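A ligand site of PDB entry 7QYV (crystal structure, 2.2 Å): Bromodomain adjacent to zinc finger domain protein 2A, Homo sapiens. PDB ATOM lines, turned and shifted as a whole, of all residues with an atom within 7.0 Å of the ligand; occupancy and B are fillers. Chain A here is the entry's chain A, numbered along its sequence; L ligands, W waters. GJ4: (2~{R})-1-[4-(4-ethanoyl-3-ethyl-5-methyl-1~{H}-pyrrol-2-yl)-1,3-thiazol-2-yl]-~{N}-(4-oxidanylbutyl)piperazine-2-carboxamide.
Water W2 lies within hydrogen-bond range of the side-chain hydroxyl (OH) of Tyr 37, an oxygen (O30) of the ligand, the backbone carbonyl oxygen (O) of Asn 75 and the backbone NH (N) of Cys 76.
The backbone carbonyl oxygen of Pro 24 is in hydrogen-bond range of a nitrogen (N24) of the ligand (2.7 Å). ND2 of Asn 80 lies within hydrogen-bond range of O30 of the ligand (2.8 Å). An oxygen (O22) of the ligand lies within hydrogen-bond range of the backbone NH (N) of Asn 30.
SG of Cys 76 is in hydrogen-bond range of O of Val 86, 3.7 Å away. ND2 of Asn 80 lies within hydrogen-bond range of O of Cys 76 (3.0 Å). The side-chain amide oxygen (OD1) of Asn 30 lies within hydrogen-bond range of the backbone NH (N) of Arg 32 (3.0 Å).
Merely in contact with the ligand: Trp 23 (3.8 Å), Phe 25 (3.8 Å), Pro 28 (3.7 Å), Val 29 (3.5 Å), Val 34 (3.7 Å), Tyr 37 (3.7 Å), Phe 79 (3.6 Å) and Val 86 (3.5 Å). Hydrophobic or aromatic side chains that line the ligand: Trp 23, Pro 24, Phe 25, Val 29, Val 34, Tyr 37, Phe 79 and Val 86. 11 residues have an atom within 4 Å of the ligand: Trp 23, Pro 24, Phe 25, Pro 28, Val 29, Asn 30, Val 34, Tyr 37, Phe 79, Asn 80 and Val 86.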
ATOM      1  N   TRP A  23      20.790  28.076 -36.666  1.00  0.00           N
ATOM      2  CA  TRP A  23      19.856  29.149 -36.369  1.00  0.00           C
ATOM      3  C   TRP A  23      18.918  28.897 -35.190  1.00  0.00           C
ATOM      4  O   TRP A  23      18.574  29.884 -34.513  1.00  0.00           O
ATOM      5  CB  TRP A  23      19.047  29.495 -37.633  1.00  0.00           C
ATOM      6  CG  TRP A  23      18.275  28.348 -38.180  1.00  0.00           C
ATOM      7  CD1 TRP A  23      18.689  27.449 -39.114  1.00  0.00           C
ATOM      8  CD2 TRP A  23      16.934  27.977 -37.835  1.00  0.00           C
ATOM      9  NE1 TRP A  23      17.697  26.536 -39.374  1.00  0.00           N
ATOM     10  CE2 TRP A  23      16.613  26.833 -38.587  1.00  0.00           C
ATOM     11  CE3 TRP A  23      15.992  28.493 -36.946  1.00  0.00           C
ATOM     12  CZ2 TRP A  23      15.375  26.201 -38.495  1.00  0.00           C
ATOM     13  CZ3 TRP A  23      14.755  27.861 -36.853  1.00  0.00           C
ATOM     14  CH2 TRP A  23      14.465  26.732 -37.628  1.00  0.00           C
ATOM     15  N   PRO A  24      18.469  27.671 -34.873  1.00  0.00           N
ATOM     16  CA  PRO A  24      17.602  27.523 -33.685  1.00  0.00           C
ATOM     17  C   PRO A  24      18.343  27.632 -32.372  1.00  0.00           C
ATOM     18  O   PRO A  24      17.698  27.733 -31.325  1.00  0.00           O
ATOM     19  CB  PRO A  24      17.001  26.121 -33.861  1.00  0.00           C
ATOM     20  CG  PRO A  24      17.347  25.689 -35.246  1.00  0.00           C
ATOM     21  CD  PRO A  24      18.637  26.374 -35.545  1.00  0.00           C
ATOM     22  N   PHE A  25      19.684  27.618 -32.375  1.00  0.00           N
ATOM     23  CA  PHE A  25      20.451  27.434 -31.156  1.00  0.00           C
ATOM     24  C   PHE A  25      21.372  28.612 -30.834  1.00  0.00           C
ATOM     25  O   PHE A  25      22.155  28.521 -29.884  1.00  0.00           O
ATOM     26  CB  PHE A  25      21.261  26.142 -31.247  1.00  0.00           C
ATOM     27  CG  PHE A  25      20.458  24.984 -31.734  1.00  0.00           C
ATOM     28  CD1 PHE A  25      19.421  24.479 -30.977  1.00  0.00           C
ATOM     29  CD2 PHE A  25      20.727  24.411 -32.972  1.00  0.00           C
ATOM     30  CE1 PHE A  25      18.668  23.413 -31.427  1.00  0.00           C
ATOM     31  CE2 PHE A  25      19.965  23.342 -33.426  1.00  0.00           C
ATOM     32  CZ  PHE A  25      18.935  22.847 -32.644  1.00  0.00           C
ATOM     33  N   LEU A  26      21.281  29.707 -31.576  1.00  0.00           N
ATOM     34  CA  LEU A  26      22.177  30.826 -31.349  1.00  0.00           C
ATOM     35  C   LEU A  26      21.808  31.631 -30.106  1.00  0.00           C
ATOM     36  O   LEU A  26      22.704  32.223 -29.489  1.00  0.00           O
ATOM     37  CB  LEU A  26      22.190  31.740 -32.578  1.00  0.00           C
ATOM     38  CG  LEU A  26      22.729  31.099 -33.868  1.00  0.00           C
ATOM     39  CD1 LEU A  26      22.524  32.013 -35.064  1.00  0.00           C
ATOM     40  CD2 LEU A  26      24.192  30.746 -33.714  1.00  0.00           C
ATOM     41  N   GLU A  27      20.548  31.656 -29.721  1.00  0.00           N
ATOM     42  CA  GLU A  27      20.068  32.390 -28.562  1.00  0.00           C
ATOM     43  C   GLU A  27      19.206  31.488 -27.694  1.00  0.00           C
ATOM     44  O   GLU A  27      18.647  30.500 -28.195  1.00  0.00           O
ATOM     45  CB  GLU A  27      19.259  33.626 -28.983  1.00  0.00           C
ATOM     46  CG  GLU A  27      20.053  34.632 -29.820  1.00  0.00           C
ATOM     47  CD  GLU A  27      21.254  35.202 -29.087  1.00  0.00           C
ATOM     48  OE1 GLU A  27      21.190  35.318 -27.846  1.00  0.00           O
ATOM     49  OE2 GLU A  27      22.261  35.530 -29.742  1.00  0.00           O
ATOM     50  N   PRO A  28      19.065  31.789 -26.405  1.00  0.00           N
ATOM     51  CA  PRO A  28      18.164  30.993 -25.560  1.00  0.00           C
ATOM     52  C   PRO A  28      16.744  31.027 -26.108  1.00  0.00           C
ATOM     53  O   PRO A  28      16.311  32.013 -26.684  1.00  0.00           O
ATOM     54  CB  PRO A  28      18.253  31.662 -24.188  1.00  0.00           C
ATOM     55  CG  PRO A  28      19.549  32.401 -24.206  1.00  0.00           C
ATOM     56  CD  PRO A  28      19.738  32.844 -25.632  1.00  0.00           C
ATOM     57  N   VAL A  29      16.031  29.916 -25.924  1.00  0.00           N
ATOM     58  CA  VAL A  29      14.619  29.882 -26.259  1.00  0.00           C
ATOM     59  C   VAL A  29      13.860  30.808 -25.307  1.00  0.00           C
ATOM     60  O   VAL A  29      14.075  30.770 -24.095  1.00  0.00           O
ATOM     61  CB  VAL A  29      14.074  28.442 -26.176  1.00  0.00           C
ATOM     62  CG1 VAL A  29      12.572  28.431 -26.379  1.00  0.00           C
ATOM     63  CG2 VAL A  29      14.772  27.547 -27.203  1.00  0.00           C
ATOM     64  N   ASN A  30      12.981  31.633 -25.866  1.00  0.00           N
ATOM     65  CA  ASN A  30      12.173  32.529 -25.046  1.00  0.00           C
ATOM     66  C   ASN A  30      10.922  31.779 -24.613  1.00  0.00           C
ATOM     67  O   ASN A  30      10.041  31.523 -25.446  1.00  0.00           O
ATOM     68  CB  ASN A  30      11.788  33.777 -25.841  1.00  0.00           C
ATOM     69  CG  ASN A  30      11.143  34.849 -24.977  1.00  0.00           C
ATOM     70  OD1 ASN A  30      10.493  34.546 -23.980  1.00  0.00           O
ATOM     71  ND2 ASN A  30      11.338  36.100 -25.355  1.00  0.00           N
ATOM     72  N   PRO A  31      10.799  31.390 -23.336  1.00  0.00           N
ATOM     73  CA  PRO A  31       9.623  30.617 -22.921  1.00  0.00           C
ATOM     74  C   PRO A  31       8.306  31.379 -23.011  1.00  0.00           C
ATOM     75  O   PRO A  31       7.246  30.750 -23.052  1.00  0.00           O
ATOM     76  CB  PRO A  31       9.939  30.228 -21.463  1.00  0.00           C
ATOM     77  CG  PRO A  31      10.911  31.266 -21.012  1.00  0.00           C
ATOM     78  CD  PRO A  31      11.728  31.647 -22.226  1.00  0.00           C
ATOM     79  N   ARG A  32       8.345  32.714 -23.059  1.00  0.00           N
ATOM     80  CA  ARG A  32       7.130  33.471 -23.291  1.00  0.00           C
ATOM     81  C   ARG A  32       6.548  33.218 -24.674  1.00  0.00           C
ATOM     82  O   ARG A  32       5.339  33.410 -24.871  1.00  0.00           O
ATOM     83  CB  ARG A  32       7.380  34.975 -23.102  1.00  0.00           C
ATOM     84  CG  ARG A  32       7.735  35.379 -21.680  1.00  0.00           C
ATOM     85  CD  ARG A  32       8.345  36.772 -21.643  1.00  0.00           C
ATOM     86  NE  ARG A  32       8.404  37.316 -20.284  1.00  0.00           N
ATOM     87  CZ  ARG A  32       8.944  38.498 -19.973  1.00  0.00           C
ATOM     88  NH1 ARG A  32       9.487  39.249 -20.932  1.00  0.00           N
ATOM     89  NH2 ARG A  32       8.953  38.914 -18.715  1.00  0.00           N
ATOM     90  N   LEU A  33       7.374  32.787 -25.630  1.00  0.00           N
ATOM     91  CA  LEU A  33       6.935  32.598 -27.006  1.00  0.00           C
ATOM     92  C   LEU A  33       6.667  31.149 -27.361  1.00  0.00           C
ATOM     93  O   LEU A  33       6.031  30.890 -28.383  1.00  0.00           O
ATOM     94  CB  LEU A  33       7.974  33.174 -27.972  1.00  0.00           C
ATOM     95  CG  LEU A  33       8.394  34.620 -27.679  1.00  0.00           C
ATOM     96  CD1 LEU A  33       9.570  35.041 -28.541  1.00  0.00           C
ATOM     97  CD2 LEU A  33       7.224  35.567 -27.873  1.00  0.00           C
ATOM     98  N   VAL A  34       7.138  30.201 -26.551  1.00  0.00           N
ATOM     99  CA  VAL A  34       7.028  28.777 -26.864  1.00  0.00           C
ATOM    100  C   VAL A  34       6.238  28.128 -25.739  1.00  0.00           C
ATOM    101  O   VAL A  34       6.765  27.879 -24.650  1.00  0.00           O
ATOM    102  CB  VAL A  34       8.400  28.113 -27.032  1.00  0.00           C
ATOM    103  CG1 VAL A  34       8.233  26.646 -27.391  1.00  0.00           C
ATOM    104  CG2 VAL A  34       9.207  28.839 -28.099  1.00  0.00           C
ATOM    105  N   TYR A  37       7.476  25.197 -22.946  1.00  0.00           N
ATOM    106  CA  TYR A  37       8.924  24.962 -22.929  1.00  0.00           C
ATOM    107  C   TYR A  37       9.456  24.919 -21.501  1.00  0.00           C
ATOM    108  O   TYR A  37      10.244  24.030 -21.151  1.00  0.00           O
ATOM    109  CB  TYR A  37       9.647  26.039 -23.737  1.00  0.00           C
ATOM    110  CG  TYR A  37      11.081  25.656 -24.049  1.00  0.00           C
ATOM    111  CD1 TYR A  37      11.371  24.830 -25.137  1.00  0.00           C
ATOM    112  CD2 TYR A  37      12.133  26.090 -23.254  1.00  0.00           C
ATOM    113  CE1 TYR A  37      12.672  24.468 -25.430  1.00  0.00           C
ATOM    114  CE2 TYR A  37      13.442  25.730 -23.542  1.00  0.00           C
ATOM    115  CZ  TYR A  37      13.705  24.915 -24.626  1.00  0.00           C
ATOM    116  OH  TYR A  37      14.997  24.540 -24.920  1.00  0.00           O
ATOM    117  N   ILE A  41      11.437  21.477 -20.480  1.00  0.00           N
ATOM    118  CA  ILE A  41      12.885  21.548 -20.530  1.00  0.00           C
ATOM    119  C   ILE A  41      13.383  22.088 -19.199  1.00  0.00           C
ATOM    120  O   ILE A  41      13.253  23.283 -18.912  1.00  0.00           O
ATOM    121  CB  ILE A  41      13.377  22.406 -21.707  1.00  0.00           C
ATOM    122  CG1 ILE A  41      13.017  21.720 -23.023  1.00  0.00           C
ATOM    123  CG2 ILE A  41      14.870  22.657 -21.605  1.00  0.00           C
ATOM    124  CD1 ILE A  41      13.595  20.324 -23.153  1.00  0.00           C
ATOM    125  N   MET A  45      19.724  25.313 -22.635  1.00  0.00           N
ATOM    126  CA  MET A  45      21.097  25.556 -23.039  1.00  0.00           C
ATOM    127  C   MET A  45      21.096  25.986 -24.496  1.00  0.00           C
ATOM    128  O   MET A  45      20.192  25.628 -25.259  1.00  0.00           O
ATOM    129  CB  MET A  45      21.971  24.311 -22.821  1.00  0.00           C
ATOM    130  CG  MET A  45      23.463  24.506 -23.034  1.00  0.00           C
ATOM    131  SD  MET A  45      24.165  25.992 -22.291  1.00  0.00           S
ATOM    132  CE  MET A  45      23.790  25.731 -20.552  1.00  0.00           C
ATOM    133  N   VAL A  72      22.223  20.821 -25.432  1.00  0.00           N
ATOM    134  CA  VAL A  72      21.471  21.561 -26.460  1.00  0.00           C
ATOM    135  C   VAL A  72      20.618  20.599 -27.294  1.00  0.00           C
ATOM    136  O   VAL A  72      19.410  20.815 -27.485  1.00  0.00           O
ATOM    137  CB  VAL A  72      22.442  22.365 -27.350  1.00  0.00           C
ATOM    138  CG1 VAL A  72      21.670  23.074 -28.456  1.00  0.00           C
ATOM    139  CG2 VAL A  72      23.229  23.372 -26.525  1.00  0.00           C
ATOM    140  N   ASN A  75      17.847  18.587 -25.338  1.00  0.00           N
ATOM    141  CA  ASN A  75      16.668  19.441 -25.211  1.00  0.00           C
ATOM    142  C   ASN A  75      15.931  19.545 -26.531  1.00  0.00           C
ATOM    143  O   ASN A  75      14.688  19.496 -26.567  1.00  0.00           O
ATOM    144  CB  ASN A  75      17.059  20.838 -24.734  1.00  0.00           C
ATOM    145  CG  ASN A  75      17.569  20.845 -23.312  1.00  0.00           C
ATOM    146  OD1 ASN A  75      17.289  19.933 -22.537  1.00  0.00           O
ATOM    147  ND2 ASN A  75      18.326  21.884 -22.961  1.00  0.00           N
ATOM    148  N   CYS A  76      16.676  19.699 -27.627  1.00  0.00           N
ATOM    149  CA  CYS A  76      16.059  19.814 -28.937  1.00  0.00           C
ATOM    150  C   CYS A  76      15.214  18.584 -29.266  1.00  0.00           C
ATOM    151  O   CYS A  76      14.070  18.695 -29.714  1.00  0.00           O
ATOM    152  CB  CYS A  76      17.140  20.010 -30.005  1.00  0.00           C
ATOM    153  SG  CYS A  76      16.463  20.155 -31.648  1.00  0.00           S
ATOM    154  N   PHE A  79      11.991  18.381 -26.995  1.00  0.00           N
ATOM    155  CA  PHE A  79      10.848  19.252 -27.220  1.00  0.00           C
ATOM    156  C   PHE A  79      10.295  19.214 -28.634  1.00  0.00           C
ATOM    157  O   PHE A  79       9.080  19.348 -28.814  1.00  0.00           O
ATOM    158  CB  PHE A  79      11.206  20.701 -26.881  1.00  0.00           C
ATOM    159  CG  PHE A  79      10.007  21.588 -26.777  1.00  0.00           C
ATOM    160  CD1 PHE A  79       9.353  21.731 -25.564  1.00  0.00           C
ATOM    161  CD2 PHE A  79       9.505  22.250 -27.880  1.00  0.00           C
ATOM    162  CE1 PHE A  79       8.247  22.528 -25.457  1.00  0.00           C
ATOM    163  CE2 PHE A  79       8.394  23.052 -27.789  1.00  0.00           C
ATOM    164  CZ  PHE A  79       7.758  23.190 -26.563  1.00  0.00           C
ATOM    165  N   ASN A  80      11.146  19.054 -29.641  1.00  0.00           N
ATOM    166  CA  ASN A  80      10.743  19.194 -31.033  1.00  0.00           C
ATOM    167  C   ASN A  80      10.629  17.833 -31.715  1.00  0.00           C
ATOM    168  O   ASN A  80      11.378  16.906 -31.402  1.00  0.00           O
ATOM    169  CB  ASN A  80      11.724  20.066 -31.804  1.00  0.00           C
ATOM    170  CG  ASN A  80      11.988  21.382 -31.097  1.00  0.00           C
ATOM    171  OD1 ASN A  80      11.214  22.335 -31.225  1.00  0.00           O
ATOM    172  ND2 ASN A  80      13.083  21.448 -30.346  1.00  0.00           N
ATOM    173  N   VAL A  86      13.005  22.821 -36.594  1.00  0.00           N
ATOM    174  CA  VAL A  86      14.023  22.921 -35.546  1.00  0.00           C
ATOM    175  C   VAL A  86      14.620  21.558 -35.255  1.00  0.00           C
ATOM    176  O   VAL A  86      15.828  21.425 -35.043  1.00  0.00           O
ATOM    177  CB  VAL A  86      13.428  23.550 -34.276  1.00  0.00           C
ATOM    178  CG1 VAL A  86      14.392  23.409 -33.119  1.00  0.00           C
ATOM    179  CG2 VAL A  86      13.089  25.015 -34.512  1.00  0.00           C
HETATM  180  C01 GJ4 L   1      10.739  26.454 -32.380  1.00  0.00           C
HETATM  181  C02 GJ4 L   1      11.431  27.426 -31.406  1.00  0.00           C
HETATM  182  C04 GJ4 L   1      14.029  27.684 -31.638  1.00  0.00           C
HETATM  183  C05 GJ4 L   1      14.034  28.835 -32.498  1.00  0.00           C
HETATM  184  C06 GJ4 L   1      14.995  29.792 -32.396  1.00  0.00           C
HETATM  185  C08 GJ4 L   1      13.171  30.119 -34.216  1.00  0.00           C
HETATM  186  N09 GJ4 L   1      12.262  30.526 -35.305  1.00  0.00           N
HETATM  187  C10 GJ4 L   1      12.117  31.904 -35.659  1.00  0.00           C
HETATM  188  C11 GJ4 L   1      11.584  32.099 -37.140  1.00  0.00           C
HETATM  189  C13 GJ4 L   1      10.167  30.381 -36.717  1.00  0.00           C
HETATM  190  C14 GJ4 L   1      10.935  29.914 -35.425  1.00  0.00           C
HETATM  191  C15 GJ4 L   1      10.105  30.270 -34.188  1.00  0.00           C
HETATM  192  C18 GJ4 L   1       9.697  31.795 -32.204  1.00  0.00           C
HETATM  193  C21 GJ4 L   1      11.760  31.682 -28.909  1.00  0.00           C
HETATM  194  C25 GJ4 L   1      14.757  26.013 -30.404  1.00  0.00           C
HETATM  195  C26 GJ4 L   1      15.708  25.038 -29.687  1.00  0.00           C
HETATM  196  C27 GJ4 L   1      13.369  25.977 -30.353  1.00  0.00           C
HETATM  197  C03 GJ4 L   1      12.891  27.049 -31.147  1.00  0.00           C
HETATM  198  C19 GJ4 L   1      10.248  31.041 -30.928  1.00  0.00           C
HETATM  199  C20 GJ4 L   1      11.625  31.587 -30.482  1.00  0.00           C
HETATM  200  C28 GJ4 L   1      12.495  24.945 -29.570  1.00  0.00           C
HETATM  201  C29 GJ4 L   1      10.997  25.181 -29.410  1.00  0.00           C
HETATM  202  N12 GJ4 L   1      10.973  30.964 -37.624  1.00  0.00           N
HETATM  203  N17 GJ4 L   1      10.487  31.452 -33.372  1.00  0.00           N
HETATM  204  N23 GJ4 L   1      13.083  29.018 -33.464  1.00  0.00           N
HETATM  205  N24 GJ4 L   1      15.114  27.046 -31.184  1.00  0.00           N
HETATM  206  O16 GJ4 L   1       9.125  29.578 -33.873  1.00  0.00           O
HETATM  207  O22 GJ4 L   1      13.125  31.973 -28.594  1.00  0.00           O
HETATM  208  O30 GJ4 L   1      12.998  23.999 -29.099  1.00  0.00           O
HETATM  209  S07 GJ4 L   1      14.561  30.983 -33.672  1.00  0.00           S
HETATM  210  O   HOH W   1      16.810  30.911 -29.990  1.00  0.00           O
HETATM  211  O   HOH W   2      15.122  22.732 -27.038  1.00  0.00           O
